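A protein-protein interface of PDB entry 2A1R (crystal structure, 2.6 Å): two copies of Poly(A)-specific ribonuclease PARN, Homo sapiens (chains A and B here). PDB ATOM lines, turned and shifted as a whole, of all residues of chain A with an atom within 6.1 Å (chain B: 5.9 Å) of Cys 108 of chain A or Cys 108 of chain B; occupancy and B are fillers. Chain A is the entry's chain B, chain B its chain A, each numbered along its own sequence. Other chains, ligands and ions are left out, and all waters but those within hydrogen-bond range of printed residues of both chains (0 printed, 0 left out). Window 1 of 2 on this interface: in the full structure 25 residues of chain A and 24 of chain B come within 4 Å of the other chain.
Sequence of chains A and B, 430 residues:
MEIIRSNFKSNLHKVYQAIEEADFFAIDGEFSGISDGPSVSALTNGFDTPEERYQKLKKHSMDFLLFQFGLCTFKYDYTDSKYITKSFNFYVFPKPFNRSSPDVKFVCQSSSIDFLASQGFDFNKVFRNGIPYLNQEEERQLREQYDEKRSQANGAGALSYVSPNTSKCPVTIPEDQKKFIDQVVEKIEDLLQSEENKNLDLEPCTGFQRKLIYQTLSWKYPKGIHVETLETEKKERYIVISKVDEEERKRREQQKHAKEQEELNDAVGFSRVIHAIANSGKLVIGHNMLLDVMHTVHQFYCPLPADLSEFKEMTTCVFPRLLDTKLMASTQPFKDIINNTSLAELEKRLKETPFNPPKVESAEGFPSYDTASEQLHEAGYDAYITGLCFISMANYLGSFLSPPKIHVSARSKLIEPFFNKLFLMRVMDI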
ATOM      1  N   SER A  32     -21.285  10.995  -4.979  1.00  0.00           N
ATOM      2  CA  SER A  32     -21.689   9.931  -4.041  1.00  0.00           C
ATOM      3  C   SER A  32     -22.951  10.303  -3.281  1.00  0.00           C
ATOM      4  O   SER A  32     -23.522   9.469  -2.590  1.00  0.00           O
ATOM      5  CB  SER A  32     -20.577   9.648  -3.033  1.00  0.00           C
ATOM      6  OG  SER A  32     -20.330  10.768  -2.201  1.00  0.00           O
ATOM      7  N   GLY A  33     -23.346  11.573  -3.398  1.00  0.00           N
ATOM      8  CA  GLY A  33     -24.559  12.109  -2.799  1.00  0.00           C
ATOM      9  C   GLY A  33     -24.647  13.630  -2.961  1.00  0.00           C
ATOM     10  O   GLY A  33     -23.841  14.251  -3.628  1.00  0.00           O
ATOM     11  N   ASP A  63     -18.763  17.054   1.701  1.00  0.00           N
ATOM     12  CA  ASP A  63     -18.203  15.815   2.208  1.00  0.00           C
ATOM     13  C   ASP A  63     -18.472  14.681   1.226  1.00  0.00           C
ATOM     14  O   ASP A  63     -17.853  13.623   1.323  1.00  0.00           O
ATOM     15  CB  ASP A  63     -18.750  15.484   3.595  1.00  0.00           C
ATOM     16  CG  ASP A  63     -18.064  16.280   4.696  1.00  0.00           C
ATOM     17  OD1 ASP A  63     -16.812  16.351   4.678  1.00  0.00           O
ATOM     18  OD2 ASP A  63     -18.692  16.857   5.617  1.00  0.00           O
ATOM     19  N   PHE A  64     -19.384  14.904   0.278  1.00  0.00           N
ATOM     20  CA  PHE A  64     -19.660  13.899  -0.738  1.00  0.00           C
ATOM     21  C   PHE A  64     -18.541  13.937  -1.767  1.00  0.00           C
ATOM     22  O   PHE A  64     -17.792  14.906  -1.845  1.00  0.00           O
ATOM     23  CB  PHE A  64     -21.005  14.122  -1.393  1.00  0.00           C
ATOM     24  CG  PHE A  64     -22.154  13.932  -0.472  1.00  0.00           C
ATOM     25  CD1 PHE A  64     -22.800  15.021   0.087  1.00  0.00           C
ATOM     26  CD2 PHE A  64     -22.599  12.667  -0.159  1.00  0.00           C
ATOM     27  CE1 PHE A  64     -23.865  14.835   0.931  1.00  0.00           C
ATOM     28  CE2 PHE A  64     -23.680  12.480   0.697  1.00  0.00           C
ATOM     29  CZ  PHE A  64     -24.310  13.557   1.230  1.00  0.00           C
ATOM     30  N   VAL A 104      -8.918   9.683   2.976  1.00  0.00           N
ATOM     31  CA  VAL A 104     -10.109  10.488   2.787  1.00  0.00           C
ATOM     32  C   VAL A 104     -11.323   9.725   3.277  1.00  0.00           C
ATOM     33  O   VAL A 104     -11.525   8.584   2.908  1.00  0.00           O
ATOM     34  CB  VAL A 104     -10.307  10.880   1.306  1.00  0.00           C
ATOM     35  CG1 VAL A 104     -11.578  11.708   1.128  1.00  0.00           C
ATOM     36  CG2 VAL A 104      -9.090  11.644   0.774  1.00  0.00           C
ATOM     37  N   LYS A 105     -12.107  10.356   4.141  1.00  0.00           N
ATOM     38  CA  LYS A 105     -13.440   9.891   4.475  1.00  0.00           C
ATOM     39  C   LYS A 105     -14.407  10.697   3.617  1.00  0.00           C
ATOM     40  O   LYS A 105     -14.341  11.911   3.570  1.00  0.00           O
ATOM     41  CB  LYS A 105     -13.758  10.153   5.940  1.00  0.00           C
ATOM     42  CG  LYS A 105     -13.339   9.057   6.921  1.00  0.00           C
ATOM     43  CD  LYS A 105     -11.819   8.856   7.025  1.00  0.00           C
ATOM     44  CE  LYS A 105     -11.075  10.107   7.449  1.00  0.00           C
ATOM     45  NZ  LYS A 105      -9.669   9.772   7.827  1.00  0.00           N
ATOM     46  N   PHE A 106     -15.304  10.028   2.926  1.00  0.00           N
ATOM     47  CA  PHE A 106     -16.337  10.735   2.212  1.00  0.00           C
ATOM     48  C   PHE A 106     -17.688  10.141   2.586  1.00  0.00           C
ATOM     49  O   PHE A 106     -17.753   9.024   3.060  1.00  0.00           O
ATOM     50  CB  PHE A 106     -16.084  10.684   0.702  1.00  0.00           C
ATOM     51  CG  PHE A 106     -16.011   9.308   0.150  1.00  0.00           C
ATOM     52  CD1 PHE A 106     -17.127   8.716  -0.411  1.00  0.00           C
ATOM     53  CD2 PHE A 106     -14.841   8.594   0.200  1.00  0.00           C
ATOM     54  CE1 PHE A 106     -17.064   7.420  -0.920  1.00  0.00           C
ATOM     55  CE2 PHE A 106     -14.779   7.302  -0.307  1.00  0.00           C
ATOM     56  CZ  PHE A 106     -15.887   6.721  -0.866  1.00  0.00           C
ATOM     57  N   VAL A 107     -18.750  10.916   2.388  1.00  0.00           N
ATOM     58  CA  VAL A 107     -20.100  10.495   2.680  1.00  0.00           C
ATOM     59  C   VAL A 107     -20.756  10.014   1.377  1.00  0.00           C
ATOM     60  O   VAL A 107     -20.521  10.527   0.285  1.00  0.00           O
ATOM     61  CB  VAL A 107     -20.924  11.646   3.345  1.00  0.00           C
ATOM     62  CG1 VAL A 107     -22.261  11.151   3.911  1.00  0.00           C
ATOM     63  CG2 VAL A 107     -20.129  12.284   4.469  1.00  0.00           C
ATOM     64  N   CYS A 108     -21.525   8.954   1.518  1.00  0.00           N
ATOM     65  CA  CYS A 108     -22.274   8.334   0.430  1.00  0.00           C
ATOM     66  C   CYS A 108     -23.766   8.569   0.837  1.00  0.00           C
ATOM     67  O   CYS A 108     -24.133   8.497   2.010  1.00  0.00           O
ATOM     68  CB  CYS A 108     -21.915   6.820   0.287  1.00  0.00           C
ATOM     69  SG  CYS A 108     -20.176   6.301  -0.050  1.00  0.00           S
ATOM     70  N   GLN A 109     -24.613   8.911  -0.122  1.00  0.00           N
ATOM     71  CA  GLN A 109     -26.041   9.099   0.154  1.00  0.00           C
ATOM     72  C   GLN A 109     -26.819   7.948  -0.466  1.00  0.00           C
ATOM     73  O   GLN A 109     -26.708   7.708  -1.662  1.00  0.00           O
ATOM     74  CB  GLN A 109     -26.542  10.417  -0.431  1.00  0.00           C
ATOM     75  CG  GLN A 109     -27.948  10.770   0.011  1.00  0.00           C
ATOM     76  CD  GLN A 109     -28.398  12.183  -0.388  1.00  0.00           C
ATOM     77  OE1 GLN A 109     -27.602  13.012  -0.793  1.00  0.00           O
ATOM     78  NE2 GLN A 109     -29.689  12.439  -0.274  1.00  0.00           N
ATOM     79  N   SER A 110     -27.604   7.249   0.344  1.00  0.00           N
ATOM     80  CA  SER A 110     -28.290   6.030  -0.079  1.00  0.00           C
ATOM     81  C   SER A 110     -29.166   6.211  -1.306  1.00  0.00           C
ATOM     82  O   SER A 110     -29.096   5.416  -2.238  1.00  0.00           O
ATOM     83  CB  SER A 110     -29.161   5.501   1.035  1.00  0.00           C
ATOM     84  OG  SER A 110     -28.363   4.807   1.968  1.00  0.00           O
ATOM     85  N   ILE A 113     -27.077   6.737  -4.428  1.00  0.00           N
ATOM     86  CA  ILE A 113     -26.405   5.523  -4.874  1.00  0.00           C
ATOM     87  C   ILE A 113     -27.434   4.671  -5.600  1.00  0.00           C
ATOM     88  O   ILE A 113     -27.155   4.114  -6.638  1.00  0.00           O
ATOM     89  CB  ILE A 113     -25.758   4.778  -3.668  1.00  0.00           C
ATOM     90  CG1 ILE A 113     -24.254   5.058  -3.606  1.00  0.00           C
ATOM     91  CG2 ILE A 113     -25.853   3.278  -3.821  1.00  0.00           C
ATOM     92  CD1 ILE A 113     -23.848   6.468  -3.543  1.00  0.00           C
ATOM     93  N   PHE A 127     -14.766   2.182  -7.194  1.00  0.00           N
ATOM     94  CA  PHE A 127     -14.178   1.635  -5.960  1.00  0.00           C
ATOM     95  C   PHE A 127     -13.102   0.569  -6.158  1.00  0.00           C
ATOM     96  O   PHE A 127     -12.423   0.212  -5.190  1.00  0.00           O
ATOM     97  CB  PHE A 127     -15.283   1.090  -5.045  1.00  0.00           C
ATOM     98  CG  PHE A 127     -16.294   2.117  -4.665  1.00  0.00           C
ATOM     99  CD1 PHE A 127     -17.583   2.040  -5.118  1.00  0.00           C
ATOM    100  CD2 PHE A 127     -15.947   3.201  -3.900  1.00  0.00           C
ATOM    101  CE1 PHE A 127     -18.514   3.016  -4.803  1.00  0.00           C
ATOM    102  CE2 PHE A 127     -16.892   4.175  -3.593  1.00  0.00           C
ATOM    103  CZ  PHE A 127     -18.167   4.062  -4.041  1.00  0.00           C
ATOM    104  N   SER B  32     -17.839  -0.218   5.429  1.00  0.00           N
ATOM    105  CA  SER B  32     -17.383   0.801   4.500  1.00  0.00           C
ATOM    106  C   SER B  32     -16.186   1.563   5.082  1.00  0.00           C
ATOM    107  O   SER B  32     -15.503   2.271   4.348  1.00  0.00           O
ATOM    108  CB  SER B  32     -18.517   1.758   4.167  1.00  0.00           C
ATOM    109  OG  SER B  32     -18.899   2.522   5.295  1.00  0.00           O
ATOM    110  N   GLY B  33     -15.945   1.383   6.388  1.00  0.00           N
ATOM    111  CA  GLY B  33     -14.784   1.928   7.080  1.00  0.00           C
ATOM    112  C   GLY B  33     -14.828   1.705   8.601  1.00  0.00           C
ATOM    113  O   GLY B  33     -15.773   1.113   9.112  1.00  0.00           O
ATOM    114  N   PHE B  64     -20.316   4.563   9.622  1.00  0.00           N
ATOM    115  CA  PHE B  64     -19.889   3.651   8.593  1.00  0.00           C
ATOM    116  C   PHE B  64     -20.932   2.563   8.488  1.00  0.00           C
ATOM    117  O   PHE B  64     -21.698   2.345   9.405  1.00  0.00           O
ATOM    118  CB  PHE B  64     -18.524   3.079   8.892  1.00  0.00           C
ATOM    119  CG  PHE B  64     -17.435   4.109   8.913  1.00  0.00           C
ATOM    120  CD1 PHE B  64     -17.023   4.679  10.110  1.00  0.00           C
ATOM    121  CD2 PHE B  64     -16.821   4.512   7.750  1.00  0.00           C
ATOM    122  CE1 PHE B  64     -16.018   5.623  10.132  1.00  0.00           C
ATOM    123  CE2 PHE B  64     -15.814   5.457   7.769  1.00  0.00           C
ATOM    124  CZ  PHE B  64     -15.406   6.013   8.956  1.00  0.00           C
ATOM    125  N   VAL B 104     -30.539   7.189   4.358  1.00  0.00           N
ATOM    126  CA  VAL B 104     -29.319   7.010   5.130  1.00  0.00           C
ATOM    127  C   VAL B 104     -28.098   7.665   4.500  1.00  0.00           C
ATOM    128  O   VAL B 104     -27.774   7.413   3.353  1.00  0.00           O
ATOM    129  CB  VAL B 104     -29.007   5.498   5.333  1.00  0.00           C
ATOM    130  CG1 VAL B 104     -27.779   5.315   6.202  1.00  0.00           C
ATOM    131  CG2 VAL B 104     -30.200   4.762   5.952  1.00  0.00           C
ATOM    132  N   LYS B 105     -27.412   8.499   5.274  1.00  0.00           N
ATOM    133  CA  LYS B 105     -26.107   9.013   4.878  1.00  0.00           C
ATOM    134  C   LYS B 105     -25.113   8.168   5.622  1.00  0.00           C
ATOM    135  O   LYS B 105     -25.136   8.148   6.833  1.00  0.00           O
ATOM    136  CB  LYS B 105     -25.917  10.487   5.276  1.00  0.00           C
ATOM    137  CG  LYS B 105     -26.315  11.515   4.191  1.00  0.00           C
ATOM    138  CD  LYS B 105     -27.826  11.533   3.922  1.00  0.00           C
ATOM    139  CE  LYS B 105     -28.599  12.046   5.126  1.00  0.00           C
ATOM    140  NZ  LYS B 105     -30.044  12.132   4.867  1.00  0.00           N
ATOM    141  N   PHE B 106     -24.255   7.449   4.914  1.00  0.00           N
ATOM    142  CA  PHE B 106     -23.186   6.725   5.554  1.00  0.00           C
ATOM    143  C   PHE B 106     -21.844   7.263   5.094  1.00  0.00           C
ATOM    144  O   PHE B 106     -21.768   7.975   4.116  1.00  0.00           O
ATOM    145  CB  PHE B 106     -23.331   5.208   5.342  1.00  0.00           C
ATOM    146  CG  PHE B 106     -23.313   4.778   3.931  1.00  0.00           C
ATOM    147  CD1 PHE B 106     -22.113   4.444   3.308  1.00  0.00           C
ATOM    148  CD2 PHE B 106     -24.503   4.673   3.208  1.00  0.00           C
ATOM    149  CE1 PHE B 106     -22.102   4.009   1.966  1.00  0.00           C
ATOM    150  CE2 PHE B 106     -24.503   4.251   1.872  1.00  0.00           C
ATOM    151  CZ  PHE B 106     -23.290   3.920   1.250  1.00  0.00           C
ATOM    152  N   VAL B 107     -20.800   6.929   5.849  1.00  0.00           N
ATOM    153  CA  VAL B 107     -19.439   7.377   5.617  1.00  0.00           C
ATOM    154  C   VAL B 107     -18.647   6.186   5.086  1.00  0.00           C
ATOM    155  O   VAL B 107     -18.822   5.060   5.509  1.00  0.00           O
ATOM    156  CB  VAL B 107     -18.810   7.885   6.951  1.00  0.00           C
ATOM    157  CG1 VAL B 107     -17.460   8.493   6.747  1.00  0.00           C
ATOM    158  CG2 VAL B 107     -19.695   8.920   7.575  1.00  0.00           C
ATOM    159  N   CYS B 108     -17.797   6.449   4.122  1.00  0.00           N
ATOM    160  CA  CYS B 108     -16.991   5.440   3.462  1.00  0.00           C
ATOM    161  C   CYS B 108     -15.540   5.883   3.764  1.00  0.00           C
ATOM    162  O   CYS B 108     -15.253   7.069   3.854  1.00  0.00           O
ATOM    163  CB  CYS B 108     -17.298   5.429   1.928  1.00  0.00           C
ATOM    164  SG  CYS B 108     -18.992   5.008   1.317  1.00  0.00           S
ATOM    165  N   GLN B 109     -14.626   4.940   3.951  1.00  0.00           N
ATOM    166  CA  GLN B 109     -13.218   5.256   4.270  1.00  0.00           C
ATOM    167  C   GLN B 109     -12.296   4.719   3.188  1.00  0.00           C
ATOM    168  O   GLN B 109     -12.259   3.527   2.962  1.00  0.00           O
ATOM    169  CB  GLN B 109     -12.815   4.656   5.619  1.00  0.00           C
ATOM    170  CG  GLN B 109     -11.435   5.094   6.087  1.00  0.00           C
ATOM    171  CD  GLN B 109     -11.097   4.647   7.498  1.00  0.00           C
ATOM    172  OE1 GLN B 109     -11.966   4.220   8.241  1.00  0.00           O
ATOM    173  NE2 GLN B 109      -9.822   4.761   7.873  1.00  0.00           N
ATOM    174  N   SER B 110     -11.557   5.614   2.536  1.00  0.00           N
ATOM    175  CA  SER B 110     -10.732   5.293   1.361  1.00  0.00           C
ATOM    176  C   SER B 110      -9.803   4.107   1.521  1.00  0.00           C
ATOM    177  O   SER B 110      -9.595   3.346   0.594  1.00  0.00           O
ATOM    178  CB  SER B 110      -9.867   6.491   0.970  1.00  0.00           C
ATOM    179  OG  SER B 110     -10.676   7.547   0.477  1.00  0.00           O
ATOM    180  N   ILE B 113     -12.001   0.869   1.642  1.00  0.00           N
ATOM    181  CA  ILE B 113     -12.452   0.544   0.301  1.00  0.00           C
ATOM    182  C   ILE B 113     -11.285  -0.072  -0.483  1.00  0.00           C
ATOM    183  O   ILE B 113     -11.431  -1.051  -1.193  1.00  0.00           O
ATOM    184  CB  ILE B 113     -13.003   1.810  -0.404  1.00  0.00           C
ATOM    185  CG1 ILE B 113     -14.525   1.930  -0.235  1.00  0.00           C
ATOM    186  CG2 ILE B 113     -12.769   1.741  -1.895  1.00  0.00           C
ATOM    187  CD1 ILE B 113     -15.043   1.883   1.177  1.00  0.00           C
ATOM    188  N   PHE B 127     -23.825  -2.054  -3.840  1.00  0.00           N
ATOM    189  CA  PHE B 127     -24.440  -0.810  -4.329  1.00  0.00           C
ATOM    190  C   PHE B 127     -25.512  -0.977  -5.413  1.00  0.00           C
ATOM    191  O   PHE B 127     -26.307  -0.062  -5.634  1.00  0.00           O
ATOM    192  CB  PHE B 127     -23.351   0.155  -4.797  1.00  0.00           C
ATOM    193  CG  PHE B 127     -22.417   0.563  -3.723  1.00  0.00           C
ATOM    194  CD1 PHE B 127     -21.057   0.443  -3.888  1.00  0.00           C
ATOM    195  CD2 PHE B 127     -22.890   1.076  -2.534  1.00  0.00           C
ATOM    196  CE1 PHE B 127     -20.182   0.833  -2.878  1.00  0.00           C
ATOM    197  CE2 PHE B 127     -22.018   1.483  -1.548  1.00  0.00           C
ATOM    198  CZ  PHE B 127     -20.671   1.358  -1.717  1.00  0.00           C
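O of Val 104 of chain B is in hydrogen-bond range of OG of Ser 110 of chain A (3.0 Å). The backbone NH (N) of Cys 108 of chain A is in hydrogen-bond range of the backbone carbonyl oxygen (O) of Phe 106 of chain B, 2.8 Å away. The backbone carbonyl oxygen of Phe 106 of chain A is in hydrogen-bond range of the backbone NH of Cys 108 of chain B (2.8 Å). The side-chain hydroxyl (OG) of Ser 110 of chain B is in hydrogen-bond range of the backbone carbonyl oxygen (O) of Val 104 of chain A (2.8 Å). The side-chain sulfur of Cys 108 of chain B forms a disulfide with the side-chain sulfur of Cys 108 of chain A, at 2.2 Å.
Of the 12 printed residues of chain B, 9 touch a printed residue of chain A. Hydrophobic or aromatic side chains of chain B within 4 Å of the printed part of chain A: Val 104, Phe 106, Val 107, Ile 113 and Phe 127. Of the 13 printed residues of chain A, 9 touch a printed residue of chain B. Printed residues of chain A that touch a printed residue of chain B: Val 104, Lys 105, Phe 106, Val 107, Cys 108, Gln 109, Ser 110, Ile 113 and Phe 127. Hydrophobic or aromatic side chains of chain A within 4 Å of the printed part of chain B: Val 104, Phe 106, Val 107, Ile 113 and Phe 127. Among the printed residues, 18 pairs touch across the chains.
Of the printed residues of chain B, Phe 106 of chain A touches Val 107 (3.5 Å) and Cys 108 (2.8 Å). Of the printed residues of chain B, Cys 108 of chain A touches Lys 105, Phe 106 and Cys 108. Of chain A, only Lys 105, Phe 106 and Cys 108 come within 4 Å of Cys 108 of chain B. Printed residues of chain A within 4 Å of Gln 109 of chain B: Val 104 and Lys 105. Of the printed residues of chain A, Ser 110 of chain B touches Val 104.
O of Ser 32 of chain A is in hydrogen-bond range of N of Gln 109 of chain A (2.8 Å). N of Gln 109 of chain B lies within hydrogen-bond range of O of Ser 32 of chain B (2.8 Å). The side-chain hydroxyl (OG) of Ser 32 of chain A lies within hydrogen-bond range of the backbone carbonyl oxygen (O) of Val 107 of chain A (2.5 Å). The backbone carbonyl oxygen of Asp 63 of chain A lies within hydrogen-bond range of the backbone NH of Val 107 of chain A (3.0 Å). OG of Ser 32 of chain B sits at hydrogen-bond distance from O of Val 107 of chain B (2.5 Å).
Val 104 of chain A touches Ser 110 of chain B, and with the chains exchanged Ser 110 of chain A touches Val 104 of chain B. Lys 105 of chain A touches Cys 108 of chain B, and with the chains exchanged Cys 108 of chain A touches Lys 105 of chain B. Val 107 of chain A touches Lys 105 of chain B, but with the chains exchanged Lys 105 of chain A does not touch Val 107 of chain B (4.1 Å). Ser 110 of chain A touches Phe 106 of chain B, but with the chains exchanged Phe 106 of chain A does not touch Ser 110 of chain B (4.2 Å). 12 positions are printed for both chains. Of the 18 pairs that touch across the chains among the printed residues, 16 have their exchanged pair printed and touching as well.
Among the printed residues, pairs that only touch across the chains: Val 107 of chain A with Phe 106 of chain B (3.2 Å), Phe 127 of chain A with Phe 127 of chain B (3.4 Å), Lys 105 of chain A with Cys 108 of chain B (3.4 Å), Phe 106 of chain A with Val 107 of chain B (3.5 Å), Cys 108 of chain A with Lys 105 of chain B (3.5 Å), Phe 127 of chain A with Ile 113 of chain B (3.6 Å), Ile 113 of chain A with Phe 127 of chain B (3.8 Å), Lys 105 of chain A with Gln 109 of chain B (3.9 Å), Ser 110 of chain A with Phe 106 of chain B (3.9 Å), Val 104 of chain A with Gln 109 of chain B (3.95 Å), Val 107 of chain A with Lys 105 of chain B (3.96 Å), Gln 109 of chain A with Val 104 of chain B (3.97 Å) and Gln 109 of chain A with Lys 105 of chain B (3.99 Å).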
